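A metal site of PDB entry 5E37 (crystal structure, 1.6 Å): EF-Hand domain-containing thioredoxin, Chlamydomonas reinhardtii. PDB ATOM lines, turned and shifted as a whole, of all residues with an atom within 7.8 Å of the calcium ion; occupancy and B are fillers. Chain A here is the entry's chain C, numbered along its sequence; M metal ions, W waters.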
ATOM      1  N   HIS A  45       0.155 -11.454   9.429  1.00  0.00           N
ATOM      2  CA  HIS A  45       1.208 -10.872   8.584  1.00  0.00           C
ATOM      3  C   HIS A  45       2.139 -11.900   7.946  1.00  0.00           C
ATOM      4  O   HIS A  45       2.149 -13.044   8.374  1.00  0.00           O
ATOM      5  CB  HIS A  45       2.043  -9.900   9.367  1.00  0.00           C
ATOM      6  CG  HIS A  45       2.782 -10.525  10.510  1.00  0.00           C
ATOM      7  ND1 HIS A  45       2.468 -10.262  11.832  1.00  0.00           N
ATOM      8  CD2 HIS A  45       3.822 -11.404  10.545  1.00  0.00           C
ATOM      9  CE1 HIS A  45       3.282 -10.956  12.620  1.00  0.00           C
ATOM     10  NE2 HIS A  45       4.099 -11.661  11.871  1.00  0.00           N
ATOM     11  N   ILE A  46       2.898 -11.444   6.930  1.00  0.00           N
ATOM     12  CA  ILE A  46       3.866 -12.277   6.215  1.00  0.00           C
ATOM     13  C   ILE A  46       5.265 -12.038   6.675  1.00  0.00           C
ATOM     14  O   ILE A  46       5.994 -11.091   6.282  1.00  0.00           O
ATOM     15  CB  ILE A  46       3.755 -12.156   4.649  1.00  0.00           C
ATOM     16  CG1 ILE A  46       2.388 -12.585   4.183  1.00  0.00           C
ATOM     17  CG2 ILE A  46       4.860 -12.985   3.932  1.00  0.00           C
ATOM     18  CD1 ILE A  46       2.137 -12.160   2.749  1.00  0.00           C
ATOM     19  N   MET A  80      12.836  -8.030   0.717  1.00  0.00           N
ATOM     20  CA  MET A  80      12.573  -7.461   2.015  1.00  0.00           C
ATOM     21  C   MET A  80      12.999  -5.991   2.075  1.00  0.00           C
ATOM     22  O   MET A  80      12.316  -5.185   2.747  1.00  0.00           O
ATOM     23  CB  MET A  80      13.310  -8.250   3.108  1.00  0.00           C
ATOM     24  CG  MET A  80      12.552  -9.435   3.694  1.00  0.00           C
ATOM     25  SD  MET A  80      10.897  -9.086   4.266  1.00  0.00           S
ATOM     26  CE  MET A  80      11.126  -7.985   5.630  1.00  0.00           C
ATOM     27  N   TYR A  83      10.082  -3.916  -0.139  1.00  0.00           N
ATOM     28  CA  TYR A  83       8.670  -3.960   0.103  1.00  0.00           C
ATOM     29  C   TYR A  83       8.247  -3.710   1.554  1.00  0.00           C
ATOM     30  O   TYR A  83       7.052  -3.409   1.814  1.00  0.00           O
ATOM     31  CB  TYR A  83       8.175  -5.293  -0.482  1.00  0.00           C
ATOM     32  CG  TYR A  83       8.382  -5.338  -1.998  1.00  0.00           C
ATOM     33  CD1 TYR A  83       7.535  -4.634  -2.832  1.00  0.00           C
ATOM     34  CD2 TYR A  83       9.437  -6.037  -2.582  1.00  0.00           C
ATOM     35  CE1 TYR A  83       7.703  -4.660  -4.215  1.00  0.00           C
ATOM     36  CE2 TYR A  83       9.619  -6.093  -3.950  1.00  0.00           C
ATOM     37  CZ  TYR A  83       8.743  -5.374  -4.776  1.00  0.00           C
ATOM     38  OH  TYR A  83       8.893  -5.386  -6.140  1.00  0.00           O
ATOM     39  N   ASP A  84       9.156  -3.862   2.526  1.00  0.00           N
ATOM     40  CA  ASP A  84       8.752  -3.585   3.913  1.00  0.00           C
ATOM     41  C   ASP A  84       8.819  -2.058   4.184  1.00  0.00           C
ATOM     42  O   ASP A  84       9.768  -1.578   4.827  1.00  0.00           O
ATOM     43  CB  ASP A  84       9.616  -4.344   4.900  1.00  0.00           C
ATOM     44  CG  ASP A  84       9.162  -4.182   6.336  1.00  0.00           C
ATOM     45  OD1 ASP A  84       7.956  -3.849   6.694  1.00  0.00           O
ATOM     46  OD2 ASP A  84      10.060  -4.550   7.127  1.00  0.00           O
ATOM     47  N   VAL A  85       7.812  -1.320   3.703  1.00  0.00           N
ATOM     48  CA  VAL A  85       7.764   0.155   3.826  1.00  0.00           C
ATOM     49  C   VAL A  85       8.146   0.544   5.266  1.00  0.00           C
ATOM     50  O   VAL A  85       9.219   1.105   5.511  1.00  0.00           O
ATOM     51  CB  VAL A  85       6.374   0.735   3.447  1.00  0.00           C
ATOM     52  CG1 VAL A  85       6.332   2.244   3.712  1.00  0.00           C
ATOM     53  CG2 VAL A  85       6.021   0.456   1.988  1.00  0.00           C
ATOM     54  N   ASN A  86       7.311   0.138   6.222  1.00  0.00           N
ATOM     55  CA  ASN A  86       7.443   0.544   7.624  1.00  0.00           C
ATOM     56  C   ASN A  86       8.517  -0.136   8.443  1.00  0.00           C
ATOM     57  O   ASN A  86       8.514  -0.023   9.659  1.00  0.00           O
ATOM     58  CB  ASN A  86       6.089   0.461   8.350  1.00  0.00           C
ATOM     59  CG  ASN A  86       5.598  -0.964   8.516  1.00  0.00           C
ATOM     60  OD1 ASN A  86       6.333  -1.848   8.949  1.00  0.00           O
ATOM     61  ND2 ASN A  86       4.345  -1.190   8.164  1.00  0.00           N
ATOM     62  N   LYS A  87       9.418  -0.852   7.779  1.00  0.00           N
ATOM     63  CA  LYS A  87      10.660  -1.411   8.355  1.00  0.00           C
ATOM     64  C   LYS A  87      10.586  -2.320   9.610  1.00  0.00           C
ATOM     65  O   LYS A  87      11.591  -2.464  10.320  1.00  0.00           O
ATOM     66  CB  LYS A  87      11.710  -0.291   8.517  1.00  0.00           C
ATOM     67  CG  LYS A  87      12.389   0.048   7.209  1.00  0.00           C
ATOM     68  CD  LYS A  87      13.898   0.244   7.352  1.00  0.00           C
ATOM     69  CE  LYS A  87      14.624  -0.141   6.064  1.00  0.00           C
ATOM     70  NZ  LYS A  87      15.865   0.649   5.880  1.00  0.00           N
ATOM     71  N   ASP A  88       9.440  -2.978   9.822  1.00  0.00           N
ATOM     72  CA  ASP A  88       9.275  -3.898  10.949  1.00  0.00           C
ATOM     73  C   ASP A  88       9.691  -5.380  10.678  1.00  0.00           C
ATOM     74  O   ASP A  88       9.516  -6.226  11.560  1.00  0.00           O
ATOM     75  CB  ASP A  88       7.860  -3.761  11.564  1.00  0.00           C
ATOM     76  CG  ASP A  88       6.741  -4.183  10.630  1.00  0.00           C
ATOM     77  OD1 ASP A  88       5.570  -4.132  11.022  1.00  0.00           O
ATOM     78  OD2 ASP A  88       7.011  -4.546   9.495  1.00  0.00           O
ATOM     79  N   GLY A  89      10.279  -5.694   9.523  1.00  0.00           N
ATOM     80  CA  GLY A  89      10.784  -7.063   9.245  1.00  0.00           C
ATOM     81  C   GLY A  89       9.730  -8.061   8.787  1.00  0.00           C
ATOM     82  O   GLY A  89       9.951  -9.282   8.773  1.00  0.00           O
ATOM     83  N   VAL A  90       8.561  -7.559   8.449  1.00  0.00           N
ATOM     84  CA  VAL A  90       7.425  -8.395   8.088  1.00  0.00           C
ATOM     85  C   VAL A  90       6.655  -7.677   6.981  1.00  0.00           C
ATOM     86  O   VAL A  90       6.876  -6.487   6.767  1.00  0.00           O
ATOM     87  CB  VAL A  90       6.505  -8.627   9.308  1.00  0.00           C
ATOM     88  CG1 VAL A  90       5.312  -9.446   8.924  1.00  0.00           C
ATOM     89  CG2 VAL A  90       7.237  -9.369  10.399  1.00  0.00           C
ATOM     90  N   ILE A  91       5.756  -8.387   6.294  1.00  0.00           N
ATOM     91  CA  ILE A  91       4.936  -7.806   5.224  1.00  0.00           C
ATOM     92  C   ILE A  91       3.467  -7.732   5.594  1.00  0.00           C
ATOM     93  O   ILE A  91       2.817  -8.748   5.851  1.00  0.00           O
ATOM     94  CB  ILE A  91       5.174  -8.618   3.903  1.00  0.00           C
ATOM     95  CG1 ILE A  91       6.677  -8.647   3.514  1.00  0.00           C
ATOM     96  CG2 ILE A  91       4.216  -8.200   2.794  1.00  0.00           C
ATOM     97  CD1 ILE A  91       7.327  -7.329   3.057  1.00  0.00           C
ATOM     98  N   SER A  92       2.921  -6.501   5.620  1.00  0.00           N
ATOM     99  CA  SER A  92       1.523  -6.283   5.878  1.00  0.00           C
ATOM    100  C   SER A  92       0.749  -6.416   4.626  1.00  0.00           C
ATOM    101  O   SER A  92       1.319  -6.493   3.563  1.00  0.00           O
ATOM    102  CB  SER A  92       1.303  -4.846   6.361  1.00  0.00           C
ATOM    103  OG  SER A  92       1.962  -3.962   5.449  1.00  0.00           O
ATOM    104  N   PHE A  93      -0.569  -6.382   4.729  1.00  0.00           N
ATOM    105  CA  PHE A  93      -1.394  -6.424   3.551  1.00  0.00           C
ATOM    106  C   PHE A  93      -1.045  -5.350   2.505  1.00  0.00           C
ATOM    107  O   PHE A  93      -1.076  -5.650   1.316  1.00  0.00           O
ATOM    108  CB  PHE A  93      -2.868  -6.417   3.901  1.00  0.00           C
ATOM    109  CG  PHE A  93      -3.742  -6.426   2.712  1.00  0.00           C
ATOM    110  CD1 PHE A  93      -3.671  -7.456   1.791  1.00  0.00           C
ATOM    111  CD2 PHE A  93      -4.661  -5.403   2.499  1.00  0.00           C
ATOM    112  CE1 PHE A  93      -4.487  -7.465   0.673  1.00  0.00           C
ATOM    113  CE2 PHE A  93      -5.480  -5.414   1.394  1.00  0.00           C
ATOM    114  CZ  PHE A  93      -5.402  -6.450   0.474  1.00  0.00           C
ATOM    115  N   GLU A  95       1.914  -3.909   1.860  1.00  0.00           N
ATOM    116  CA  GLU A  95       3.176  -4.101   1.220  1.00  0.00           C
ATOM    117  C   GLU A  95       3.153  -5.348   0.339  1.00  0.00           C
ATOM    118  O   GLU A  95       3.951  -5.435  -0.617  1.00  0.00           O
ATOM    119  CB  GLU A  95       4.256  -4.264   2.273  1.00  0.00           C
ATOM    120  CG  GLU A  95       4.352  -3.054   3.208  1.00  0.00           C
ATOM    121  CD  GLU A  95       4.810  -3.393   4.631  1.00  0.00           C
ATOM    122  OE1 GLU A  95       4.926  -4.594   5.014  1.00  0.00           O
ATOM    123  OE2 GLU A  95       5.046  -2.429   5.390  1.00  0.00           O
HETATM  124 CA    CA M   1       5.993  -4.024   7.349  1.00  0.00          CA
HETATM  125  O   HOH W   1       4.022  -4.096   8.318  1.00  0.00           O
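The calcium ion is bound by the side-chain carboxylate (OD1) of Asp 84, water W1, the side-chain carboxylate (OD2) of Asp 88, the side-chain carboxylate (OE1) of Glu 95, the backbone carbonyl oxygen (O) of Val 90, the side-chain carboxylate (OE2) of Glu 95 and the side-chain amide oxygen (OD1) of Asn 86.
The calcium ion has seven donor atoms within binding distance.
Water W1 bridges the side-chain amide nitrogen of Asn 86 and the side-chain carboxylate of Asp 88.
The side-chain carboxylate (OE1) of Glu 95 lies close to the backbone NH (N) of Ser 92.
N of Gly 89 is in hydrogen-bond range of OD2 of Asp 84 (2.7 Å).
OE2 of Glu 95 sits close to N of Val 85.
Five residues have an atom within 4 Å of the calcium ion: Asp 84, Asn 86, Asp 88, Val 90 and Glu 95.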
